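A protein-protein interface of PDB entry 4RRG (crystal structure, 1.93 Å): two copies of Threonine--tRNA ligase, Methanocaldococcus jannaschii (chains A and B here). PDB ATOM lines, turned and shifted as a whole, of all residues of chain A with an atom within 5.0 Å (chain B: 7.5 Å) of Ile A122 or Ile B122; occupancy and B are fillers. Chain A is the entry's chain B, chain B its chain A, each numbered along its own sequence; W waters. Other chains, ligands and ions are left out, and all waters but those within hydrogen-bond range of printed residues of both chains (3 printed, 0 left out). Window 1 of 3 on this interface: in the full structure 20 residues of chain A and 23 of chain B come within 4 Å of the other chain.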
ATOM      1  N   ILE A   6       6.436  -6.144  22.022  1.00  0.00           N
ATOM      2  CA  ILE A   6       5.848  -4.825  22.297  1.00  0.00           C
ATOM      3  C   ILE A   6       5.253  -4.774  23.709  1.00  0.00           C
ATOM      4  O   ILE A   6       4.338  -5.526  24.045  1.00  0.00           O
ATOM      5  CB  ILE A   6       4.821  -4.383  21.215  1.00  0.00           C
ATOM      6  CG1 ILE A   6       5.466  -4.412  19.815  1.00  0.00           C
ATOM      7  CG2 ILE A   6       4.308  -2.986  21.507  1.00  0.00           C
ATOM      8  CD1 ILE A   6       4.496  -4.197  18.687  1.00  0.00           C
ATOM      9  N   SER A   8       2.903  -3.456  26.086  1.00  0.00           N
ATOM     10  CA  SER A   8       1.605  -2.896  25.749  1.00  0.00           C
ATOM     11  C   SER A   8       0.727  -2.642  26.968  1.00  0.00           C
ATOM     12  O   SER A   8       0.788  -3.383  27.941  1.00  0.00           O
ATOM     13  CB  SER A   8       0.868  -3.841  24.792  1.00  0.00           C
ATOM     14  OG  SER A   8       1.683  -4.174  23.689  1.00  0.00           O
ATOM     15  N   TYR A  10      -2.462  -2.916  26.507  1.00  0.00           N
ATOM     16  CA  TYR A  10      -3.317  -4.086  26.227  1.00  0.00           C
ATOM     17  C   TYR A  10      -3.032  -4.674  24.856  1.00  0.00           C
ATOM     18  O   TYR A  10      -2.494  -4.000  23.970  1.00  0.00           O
ATOM     19  CB  TYR A  10      -4.823  -3.744  26.309  1.00  0.00           C
ATOM     20  CG  TYR A  10      -5.211  -2.576  25.446  1.00  0.00           C
ATOM     21  CD1 TYR A  10      -5.467  -2.742  24.084  1.00  0.00           C
ATOM     22  CD2 TYR A  10      -5.282  -1.291  25.981  1.00  0.00           C
ATOM     23  CE1 TYR A  10      -5.786  -1.657  23.277  1.00  0.00           C
ATOM     24  CE2 TYR A  10      -5.615  -0.203  25.189  1.00  0.00           C
ATOM     25  CZ  TYR A  10      -5.860  -0.394  23.840  1.00  0.00           C
ATOM     26  OH  TYR A  10      -6.187   0.680  23.049  1.00  0.00           O
ATOM     27  N   LEU A  11      -3.408  -5.937  24.696  1.00  0.00           N
ATOM     28  CA  LEU A  11      -3.593  -6.530  23.390  1.00  0.00           C
ATOM     29  C   LEU A  11      -4.934  -7.261  23.419  1.00  0.00           C
ATOM     30  O   LEU A  11      -5.187  -8.040  24.336  1.00  0.00           O
ATOM     31  CB  LEU A  11      -2.452  -7.499  23.071  1.00  0.00           C
ATOM     32  CG  LEU A  11      -2.379  -8.219  21.710  1.00  0.00           C
ATOM     33  CD1 LEU A  11      -3.364  -9.415  21.605  1.00  0.00           C
ATOM     34  CD2 LEU A  11      -2.563  -7.261  20.534  1.00  0.00           C
ATOM     35  N   ALA A  37       3.558  -8.175  24.148  1.00  0.00           N
ATOM     36  CA  ALA A  37       2.943  -8.749  22.963  1.00  0.00           C
ATOM     37  C   ALA A  37       4.039  -9.210  22.008  1.00  0.00           C
ATOM     38  O   ALA A  37       4.801  -8.390  21.465  1.00  0.00           O
ATOM     39  CB  ALA A  37       2.028  -7.742  22.299  1.00  0.00           C
ATOM     40  N   PHE A  39       5.026 -10.762  18.750  1.00  0.00           N
ATOM     41  CA  PHE A  39       4.697 -11.086  17.361  1.00  0.00           C
ATOM     42  C   PHE A  39       5.794 -11.949  16.769  1.00  0.00           C
ATOM     43  O   PHE A  39       6.947 -11.545  16.733  1.00  0.00           O
ATOM     44  CB  PHE A  39       4.476  -9.787  16.587  1.00  0.00           C
ATOM     45  CG  PHE A  39       3.334  -8.975  17.119  1.00  0.00           C
ATOM     46  CD1 PHE A  39       2.054  -9.111  16.576  1.00  0.00           C
ATOM     47  CD2 PHE A  39       3.528  -8.091  18.179  1.00  0.00           C
ATOM     48  CE1 PHE A  39       0.987  -8.372  17.081  1.00  0.00           C
ATOM     49  CE2 PHE A  39       2.482  -7.361  18.701  1.00  0.00           C
ATOM     50  CZ  PHE A  39       1.206  -7.480  18.147  1.00  0.00           C
ATOM     51  N   PHE A 120      -7.506  -6.989  15.638  1.00  0.00           N
ATOM     52  CA  PHE A 120      -6.835  -6.806  16.921  1.00  0.00           C
ATOM     53  C   PHE A 120      -6.702  -5.343  17.288  1.00  0.00           C
ATOM     54  O   PHE A 120      -6.828  -4.466  16.431  1.00  0.00           O
ATOM     55  CB  PHE A 120      -5.479  -7.557  16.988  1.00  0.00           C
ATOM     56  CG  PHE A 120      -4.390  -6.951  16.143  1.00  0.00           C
ATOM     57  CD1 PHE A 120      -3.531  -5.984  16.672  1.00  0.00           C
ATOM     58  CD2 PHE A 120      -4.209  -7.360  14.826  1.00  0.00           C
ATOM     59  CE1 PHE A 120      -2.507  -5.428  15.886  1.00  0.00           C
ATOM     60  CE2 PHE A 120      -3.199  -6.812  14.040  1.00  0.00           C
ATOM     61  CZ  PHE A 120      -2.348  -5.842  14.568  1.00  0.00           C
ATOM     62  N   LYS A 121      -6.477  -5.095  18.574  1.00  0.00           N
ATOM     63  CA  LYS A 121      -6.226  -3.757  19.084  1.00  0.00           C
ATOM     64  C   LYS A 121      -5.011  -3.858  19.984  1.00  0.00           C
ATOM     65  O   LYS A 121      -4.878  -4.813  20.744  1.00  0.00           O
ATOM     66  CB  LYS A 121      -7.406  -3.229  19.905  1.00  0.00           C
ATOM     67  CG  LYS A 121      -8.719  -3.088  19.154  1.00  0.00           C
ATOM     68  CD  LYS A 121      -9.754  -2.350  20.003  1.00  0.00           C
ATOM     69  CE  LYS A 121     -11.032  -2.070  19.215  1.00  0.00           C
ATOM     70  NZ  LYS A 121     -12.061  -1.384  20.063  1.00  0.00           N
ATOM     71  N   ILE A 122      -4.125  -2.875  19.885  1.00  0.00           N
ATOM     72  CA  ILE A 122      -2.938  -2.822  20.735  1.00  0.00           C
ATOM     73  C   ILE A 122      -2.652  -1.376  21.123  1.00  0.00           C
ATOM     74  O   ILE A 122      -3.003  -0.443  20.389  1.00  0.00           O
ATOM     75  CB  ILE A 122      -1.701  -3.491  20.043  1.00  0.00           C
ATOM     76  CG1 ILE A 122      -0.588  -3.795  21.054  1.00  0.00           C
ATOM     77  CG2 ILE A 122      -1.181  -2.642  18.884  1.00  0.00           C
ATOM     78  CD1 ILE A 122       0.588  -4.590  20.470  1.00  0.00           C
ATOM     79  N   SER A 123      -2.042  -1.194  22.288  1.00  0.00           N
ATOM     80  CA  SER A 123      -1.557   0.119  22.710  1.00  0.00           C
ATOM     81  C   SER A 123      -0.136  -0.054  23.218  1.00  0.00           C
ATOM     82  O   SER A 123       0.071  -0.684  24.241  1.00  0.00           O
ATOM     83  CB  SER A 123      -2.450   0.725  23.805  1.00  0.00           C
ATOM     84  OG  SER A 123      -1.976   2.015  24.183  1.00  0.00           O
ATOM     85  N   CYS A 124       0.830   0.486  22.473  1.00  0.00           N
ATOM     86  CA  CYS A 124       2.250   0.389  22.808  1.00  0.00           C
ATOM     87  C   CYS A 124       2.615   1.533  23.741  1.00  0.00           C
ATOM     88  O   CYS A 124       2.259   2.688  23.478  1.00  0.00           O
ATOM     89  CB  CYS A 124       3.105   0.504  21.542  1.00  0.00           C
ATOM     90  SG  CYS A 124       4.894   0.680  21.862  1.00  0.00           S
ATOM     91  N   LEU B   5       1.323  -3.086   5.702  1.00  0.00           N
ATOM     92  CA  LEU B   5       0.130  -2.258   5.520  1.00  0.00           C
ATOM     93  C   LEU B   5      -0.996  -2.811   6.372  1.00  0.00           C
ATOM     94  O   LEU B   5      -1.412  -3.957   6.188  1.00  0.00           O
ATOM     95  CB  LEU B   5      -0.302  -2.200   4.045  1.00  0.00           C
ATOM     96  CG  LEU B   5       0.742  -1.767   3.014  1.00  0.00           C
ATOM     97  CD1 LEU B   5       0.076  -1.290   1.747  1.00  0.00           C
ATOM     98  CD2 LEU B   5       1.491  -0.629   3.589  1.00  0.00           C
ATOM     99  N   ILE B   6      -1.470  -2.001   7.314  1.00  0.00           N
ATOM    100  CA  ILE B   6      -2.533  -2.433   8.213  1.00  0.00           C
ATOM    101  C   ILE B   6      -3.783  -1.593   8.005  1.00  0.00           C
ATOM    102  O   ILE B   6      -3.798  -0.384   8.277  1.00  0.00           O
ATOM    103  CB  ILE B   6      -2.090  -2.474   9.698  1.00  0.00           C
ATOM    104  CG1 ILE B   6      -0.815  -3.339   9.847  1.00  0.00           C
ATOM    105  CG2 ILE B   6      -3.216  -3.040  10.575  1.00  0.00           C
ATOM    106  CD1 ILE B   6      -0.224  -3.436  11.268  1.00  0.00           C
ATOM    107  N   HIS B   7      -4.834  -2.240   7.511  1.00  0.00           N
ATOM    108  CA  HIS B   7      -6.112  -1.536   7.340  1.00  0.00           C
ATOM    109  C   HIS B   7      -6.773  -1.397   8.705  1.00  0.00           C
ATOM    110  O   HIS B   7      -7.174  -2.387   9.329  1.00  0.00           O
ATOM    111  CB  HIS B   7      -7.006  -2.215   6.298  1.00  0.00           C
ATOM    112  CG  HIS B   7      -8.195  -1.395   5.898  1.00  0.00           C
ATOM    113  ND1 HIS B   7      -9.378  -1.958   5.468  1.00  0.00           N
ATOM    114  CD2 HIS B   7      -8.396  -0.055   5.900  1.00  0.00           C
ATOM    115  CE1 HIS B   7     -10.244  -0.999   5.189  1.00  0.00           C
ATOM    116  NE2 HIS B   7      -9.677   0.165   5.455  1.00  0.00           N
ATOM    117  N   SER B   8      -6.860  -0.154   9.168  1.00  0.00           N
ATOM    118  CA  SER B   8      -7.107   0.128  10.575  1.00  0.00           C
ATOM    119  C   SER B   8      -8.343   0.989  10.821  1.00  0.00           C
ATOM    120  O   SER B   8      -8.632   1.898  10.034  1.00  0.00           O
ATOM    121  CB  SER B   8      -5.887   0.845  11.156  1.00  0.00           C
ATOM    122  OG  SER B   8      -4.710   0.085  10.935  1.00  0.00           O
ATOM    123  N   ASP B   9      -9.050   0.706  11.920  1.00  0.00           N
ATOM    124  CA  ASP B   9     -10.152   1.562  12.402  1.00  0.00           C
ATOM    125  C   ASP B   9      -9.649   2.956  12.753  1.00  0.00           C
ATOM    126  O   ASP B   9     -10.336   3.955  12.522  1.00  0.00           O
ATOM    127  CB  ASP B   9     -10.819   0.941  13.639  1.00  0.00           C
ATOM    128  CG  ASP B   9     -11.447  -0.394  13.342  1.00  0.00           C
ATOM    129  OD1 ASP B   9     -12.225  -0.474  12.371  1.00  0.00           O
ATOM    130  OD2 ASP B   9     -11.159  -1.366  14.071  1.00  0.00           O
ATOM    131  N   TYR B  10      -8.432   3.000  13.303  1.00  0.00           N
ATOM    132  CA  TYR B  10      -7.774   4.225  13.731  1.00  0.00           C
ATOM    133  C   TYR B  10      -6.287   3.964  13.972  1.00  0.00           C
ATOM    134  O   TYR B  10      -5.875   2.821  14.175  1.00  0.00           O
ATOM    135  CB  TYR B  10      -8.398   4.757  15.029  1.00  0.00           C
ATOM    136  CG  TYR B  10      -8.364   3.774  16.178  1.00  0.00           C
ATOM    137  CD1 TYR B  10      -7.197   3.582  16.931  1.00  0.00           C
ATOM    138  CD2 TYR B  10      -9.503   3.045  16.530  1.00  0.00           C
ATOM    139  CE1 TYR B  10      -7.160   2.670  17.988  1.00  0.00           C
ATOM    140  CE2 TYR B  10      -9.482   2.142  17.597  1.00  0.00           C
ATOM    141  CZ  TYR B  10      -8.309   1.959  18.316  1.00  0.00           C
ATOM    142  OH  TYR B  10      -8.282   1.064  19.350  1.00  0.00           O
ATOM    143  N   LEU B  11      -5.506   5.037  13.952  1.00  0.00           N
ATOM    144  CA  LEU B  11      -4.132   5.018  14.433  1.00  0.00           C
ATOM    145  C   LEU B  11      -3.874   6.338  15.140  1.00  0.00           C
ATOM    146  O   LEU B  11      -4.126   7.418  14.583  1.00  0.00           O
ATOM    147  CB  LEU B  11      -3.128   4.799  13.297  1.00  0.00           C
ATOM    148  CG  LEU B  11      -1.648   4.667  13.703  1.00  0.00           C
ATOM    149  CD1 LEU B  11      -0.938   3.705  12.803  1.00  0.00           C
ATOM    150  CD2 LEU B  11      -0.922   6.019  13.720  1.00  0.00           C
ATOM    151  N   GLU B  12      -3.396   6.247  16.372  1.00  0.00           N
ATOM    152  CA  GLU B  12      -2.930   7.428  17.089  1.00  0.00           C
ATOM    153  C   GLU B  12      -1.525   7.187  17.586  1.00  0.00           C
ATOM    154  O   GLU B  12      -1.157   6.057  17.878  1.00  0.00           O
ATOM    155  CB  GLU B  12      -3.868   7.801  18.251  1.00  0.00           C
ATOM    156  CG  GLU B  12      -4.186   6.675  19.210  1.00  0.00           C
ATOM    157  CD  GLU B  12      -5.433   6.941  20.052  1.00  0.00           C
ATOM    158  OE1 GLU B  12      -5.566   8.052  20.619  1.00  0.00           O
ATOM    159  OE2 GLU B  12      -6.276   6.022  20.153  1.00  0.00           O
ATOM    160  N   CYS B  35      -7.905   4.055   8.242  1.00  0.00           N
ATOM    161  CA  CYS B  35      -6.734   4.373   7.437  1.00  0.00           C
ATOM    162  C   CYS B  35      -5.932   3.134   7.048  1.00  0.00           C
ATOM    163  O   CYS B  35      -6.181   2.031   7.535  1.00  0.00           O
ATOM    164  CB  CYS B  35      -5.833   5.352   8.196  1.00  0.00           C
ATOM    165  SG  CYS B  35      -5.207   4.749   9.796  1.00  0.00           S
ATOM    166  N   LEU B  36      -4.984   3.329   6.140  1.00  0.00           N
ATOM    167  CA  LEU B  36      -4.011   2.306   5.842  1.00  0.00           C
ATOM    168  C   LEU B  36      -2.745   2.725   6.572  1.00  0.00           C
ATOM    169  O   LEU B  36      -2.072   3.674   6.178  1.00  0.00           O
ATOM    170  CB  LEU B  36      -3.781   2.194   4.333  1.00  0.00           C
ATOM    171  CG  LEU B  36      -3.065   0.941   3.835  1.00  0.00           C
ATOM    172  CD1 LEU B  36      -3.906  -0.312   4.089  1.00  0.00           C
ATOM    173  CD2 LEU B  36      -2.739   1.071   2.351  1.00  0.00           C
ATOM    174  N   ALA B  37      -2.446   2.033   7.666  1.00  0.00           N
ATOM    175  CA  ALA B  37      -1.252   2.325   8.440  1.00  0.00           C
ATOM    176  C   ALA B  37      -0.110   1.577   7.761  1.00  0.00           C
ATOM    177  O   ALA B  37      -0.098   0.346   7.718  1.00  0.00           O
ATOM    178  CB  ALA B  37      -1.426   1.882   9.869  1.00  0.00           C
ATOM    179  N   CYS B  38       0.813   2.345   7.198  1.00  0.00           N
ATOM    180  CA  CYS B  38       1.940   1.813   6.461  1.00  0.00           C
ATOM    181  C   CYS B  38       3.195   1.935   7.310  1.00  0.00           C
ATOM    182  O   CYS B  38       3.751   3.019   7.471  1.00  0.00           O
ATOM    183  CB  CYS B  38       2.089   2.554   5.123  1.00  0.00           C
ATOM    184  SG  CYS B  38       0.575   2.416   4.120  1.00  0.00           S
ATOM    185  N   PHE B  39       3.615   0.807   7.862  1.00  0.00           N
ATOM    186  CA  PHE B  39       4.825   0.745   8.670  1.00  0.00           C
ATOM    187  C   PHE B  39       5.971   0.446   7.727  1.00  0.00           C
ATOM    188  O   PHE B  39       5.955  -0.569   7.033  1.00  0.00           O
ATOM    189  CB  PHE B  39       4.679  -0.327   9.746  1.00  0.00           C
ATOM    190  CG  PHE B  39       3.603  -0.020  10.760  1.00  0.00           C
ATOM    191  CD1 PHE B  39       3.911   0.652  11.930  1.00  0.00           C
ATOM    192  CD2 PHE B  39       2.286  -0.417  10.539  1.00  0.00           C
ATOM    193  CE1 PHE B  39       2.924   0.944  12.878  1.00  0.00           C
ATOM    194  CE2 PHE B  39       1.290  -0.125  11.462  1.00  0.00           C
ATOM    195  CZ  PHE B  39       1.601   0.546  12.638  1.00  0.00           C
ATOM    196  N   TYR B  76       4.368   5.500   8.718  1.00  0.00           N
ATOM    197  CA  TYR B  76       4.866   5.274  10.070  1.00  0.00           C
ATOM    198  C   TYR B  76       6.236   4.613   9.998  1.00  0.00           C
ATOM    199  O   TYR B  76       6.333   3.448   9.625  1.00  0.00           O
ATOM    200  CB  TYR B  76       3.878   4.402  10.849  1.00  0.00           C
ATOM    201  CG  TYR B  76       4.031   4.477  12.361  1.00  0.00           C
ATOM    202  CD1 TYR B  76       5.137   3.911  13.003  1.00  0.00           C
ATOM    203  CD2 TYR B  76       3.054   5.083  13.147  1.00  0.00           C
ATOM    204  CE1 TYR B  76       5.275   3.965  14.389  1.00  0.00           C
ATOM    205  CE2 TYR B  76       3.183   5.151  14.546  1.00  0.00           C
ATOM    206  CZ  TYR B  76       4.293   4.585  15.156  1.00  0.00           C
ATOM    207  OH  TYR B  76       4.430   4.653  16.529  1.00  0.00           O
ATOM    208  N   PHE B 120       1.758   4.301  20.703  1.00  0.00           N
ATOM    209  CA  PHE B 120       0.756   4.282  19.650  1.00  0.00           C
ATOM    210  C   PHE B 120      -0.366   3.311  19.948  1.00  0.00           C
ATOM    211  O   PHE B 120      -0.213   2.393  20.746  1.00  0.00           O
ATOM    212  CB  PHE B 120       1.374   4.017  18.260  1.00  0.00           C
ATOM    213  CG  PHE B 120       1.822   2.594  18.036  1.00  0.00           C
ATOM    214  CD1 PHE B 120       3.127   2.210  18.336  1.00  0.00           C
ATOM    215  CD2 PHE B 120       0.947   1.650  17.489  1.00  0.00           C
ATOM    216  CE1 PHE B 120       3.557   0.895  18.113  1.00  0.00           C
ATOM    217  CE2 PHE B 120       1.363   0.326  17.262  1.00  0.00           C
ATOM    218  CZ  PHE B 120       2.676  -0.048  17.580  1.00  0.00           C
ATOM    219  N   LYS B 121      -1.501   3.549  19.299  1.00  0.00           N
ATOM    220  CA  LYS B 121      -2.674   2.698  19.432  1.00  0.00           C
ATOM    221  C   LYS B 121      -3.172   2.429  18.034  1.00  0.00           C
ATOM    222  O   LYS B 121      -3.324   3.362  17.232  1.00  0.00           O
ATOM    223  CB  LYS B 121      -3.769   3.393  20.248  1.00  0.00           C
ATOM    224  CG  LYS B 121      -3.334   3.828  21.654  1.00  0.00           C
ATOM    225  CD  LYS B 121      -4.499   4.431  22.450  1.00  0.00           C
ATOM    226  CE  LYS B 121      -4.018   5.052  23.759  1.00  0.00           C
ATOM    227  NZ  LYS B 121      -3.243   6.311  23.519  1.00  0.00           N
ATOM    228  N   ILE B 122      -3.399   1.154  17.737  1.00  0.00           N
ATOM    229  CA  ILE B 122      -3.913   0.739  16.436  1.00  0.00           C
ATOM    230  C   ILE B 122      -4.992  -0.344  16.604  1.00  0.00           C
ATOM    231  O   ILE B 122      -4.939  -1.144  17.526  1.00  0.00           O
ATOM    232  CB  ILE B 122      -2.759   0.284  15.486  1.00  0.00           C
ATOM    233  CG1 ILE B 122      -3.234   0.214  14.031  1.00  0.00           C
ATOM    234  CG2 ILE B 122      -2.089  -1.008  15.972  1.00  0.00           C
ATOM    235  CD1 ILE B 122      -2.129  -0.069  13.032  1.00  0.00           C
ATOM    236  N   SER B 123      -5.979  -0.333  15.712  1.00  0.00           N
ATOM    237  CA  SER B 123      -7.007  -1.361  15.677  1.00  0.00           C
ATOM    238  C   SER B 123      -7.127  -1.891  14.245  1.00  0.00           C
ATOM    239  O   SER B 123      -7.576  -1.178  13.350  1.00  0.00           O
ATOM    240  CB  SER B 123      -8.333  -0.787  16.196  1.00  0.00           C
ATOM    241  OG  SER B 123      -9.418  -1.671  15.974  1.00  0.00           O
ATOM    242  N   CYS B 124      -6.686  -3.132  14.035  1.00  0.00           N
ATOM    243  CA  CYS B 124      -6.758  -3.782  12.727  1.00  0.00           C
ATOM    244  C   CYS B 124      -8.154  -4.333  12.478  1.00  0.00           C
ATOM    245  O   CYS B 124      -8.741  -4.976  13.353  1.00  0.00           O
ATOM    246  CB  CYS B 124      -5.739  -4.917  12.642  1.00  0.00           C
ATOM    247  SG  CYS B 124      -5.789  -5.837  11.109  1.00  0.00           S
ATOM    248  N   LYS B 125      -8.671  -4.087  11.277  1.00  0.00           N
ATOM    249  CA  LYS B 125     -10.038  -4.486  10.932  1.00  0.00           C
ATOM    250  C   LYS B 125     -10.216  -6.001  10.867  1.00  0.00           C
ATOM    251  O   LYS B 125     -11.271  -6.510  11.231  1.00  0.00           O
ATOM    252  CB  LYS B 125     -10.502  -3.804   9.640  1.00  0.00           C
ATOM    253  CG  LYS B 125     -10.682  -2.291   9.802  1.00  0.00           C
ATOM    254  CD  LYS B 125     -11.454  -1.673   8.653  1.00  0.00           C
ATOM    255  CE  LYS B 125     -11.724  -0.198   8.923  1.00  0.00           C
ATOM    256  NZ  LYS B 125     -12.785   0.373   8.031  1.00  0.00           N
HETATM  257  O   HOH W   1     -10.153  -4.260  16.129  1.00  0.00           O
HETATM  258  O   HOH W   2      -5.912   0.402  20.306  1.00  0.00           O
HETATM  259  O   HOH W   3      -0.570   4.103  23.683  1.00  0.00           O
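Water W3 lies within hydrogen-bond range of the side-chain hydroxyl (OG) of Ser A123, the backbone carbonyl oxygen (O) of Cys A124, the backbone carbonyl oxygen (O) of Phe B120 and the side-chain amino group (NZ) of Lys B121.
Water W2 lies within hydrogen-bond range of OH of Tyr B10, OH of Tyr A10, O of Ile A122 and O of Ile B122.
Water W1 lies within hydrogen-bond range of the side-chain hydroxyl of Ser B123 (2.7 Å), the backbone carbonyl oxygen of Cys B124 (3.2 Å) and the backbone carbonyl oxygen of Phe A120 (3.3 Å).
The backbone NH (N) of Lys B121 sits at hydrogen-bond distance from the backbone carbonyl oxygen (O) of Glu B12, 2.9 Å away.
The backbone carbonyl oxygen (O) of Tyr A10 lies within hydrogen-bond range of the backbone NH (N) of Ser A123, 3.3 Å away.
The side-chain carboxylate (OD2) of Asp B9 is in hydrogen-bond range of the side-chain hydroxyl (OG) of Ser B123, 2.6 Å away.
Of the 11 printed residues of chain A, 5 touch a printed residue of chain B.
Hydrophobic or aromatic side chains of chain A that line the printed part of chain B: Phe A120 and Ile A122.
Of the 20 printed residues of chain B, 6 touch a printed residue of chain A.
Among the printed residues, 12 pairs touch across the chains.
Phe A120 touches Cys B124, and with the chains exchanged Cys A124 touches Phe B120.
Lys A121 touches Tyr B10, but with the chains exchanged Tyr A10 does not touch Lys B121 (4.2 Å).
Lys A121 touches Ile B122, and with the chains exchanged Ile A122 touches Lys B121.
Ile B122 touches its own counterpart, Ile A122.
Positions printed for both chains: 6, 8, 10, 11, 37, 39, 120, 121, 122, 123 and 124.
The backbone carbonyl oxygen (O) of Phe A120 sits at hydrogen-bond distance from the backbone NH (N) of Cys B124, 2.7 Å away.
O of Ile B122 lies within hydrogen-bond range of N of Ile A122 (3.0 Å).
O of Phe B120 sits at hydrogen-bond distance from N of Cys A124 (2.8 Å).
Among the printed residues, pairs that only touch across the chains: Phe A120 with Ser B123, Ser A123 with Phe B120, Ile A122 with Lys B121, Lys A121 with Ile B122, Ser A123 with Lys B121, Lys A121 with Ser B123, Lys A121 with Tyr B10, Phe A120 with Ile B122 and Ile A122 with Phe B120.
Of the printed residues of chain B, Phe A120 touches Ile B122 (3.98 Å), Ser B123 (3.2 Å) and Cys B124 (2.7 Å).
Printed residues of chain B within 4 Å of Ile A122: Phe B120, Lys B121 and Ile B122.
Printed residues of chain A within 4 Å of Lys B121: Ile A122 and Ser A123.
Of the printed residues of chain A, Ile B122 touches Phe A120, Lys A121 and Ile A122.
Of the printed residues of chain A, Ser B123 touches Phe A120 (3.2 Å) and Lys A121 (3.6 Å).
Of the printed residues of chain A, Cys B124 touches Phe A120.
The nearest printed residue of chain A that does not touch Ile B122 is Ser A123 (5.3 Å).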
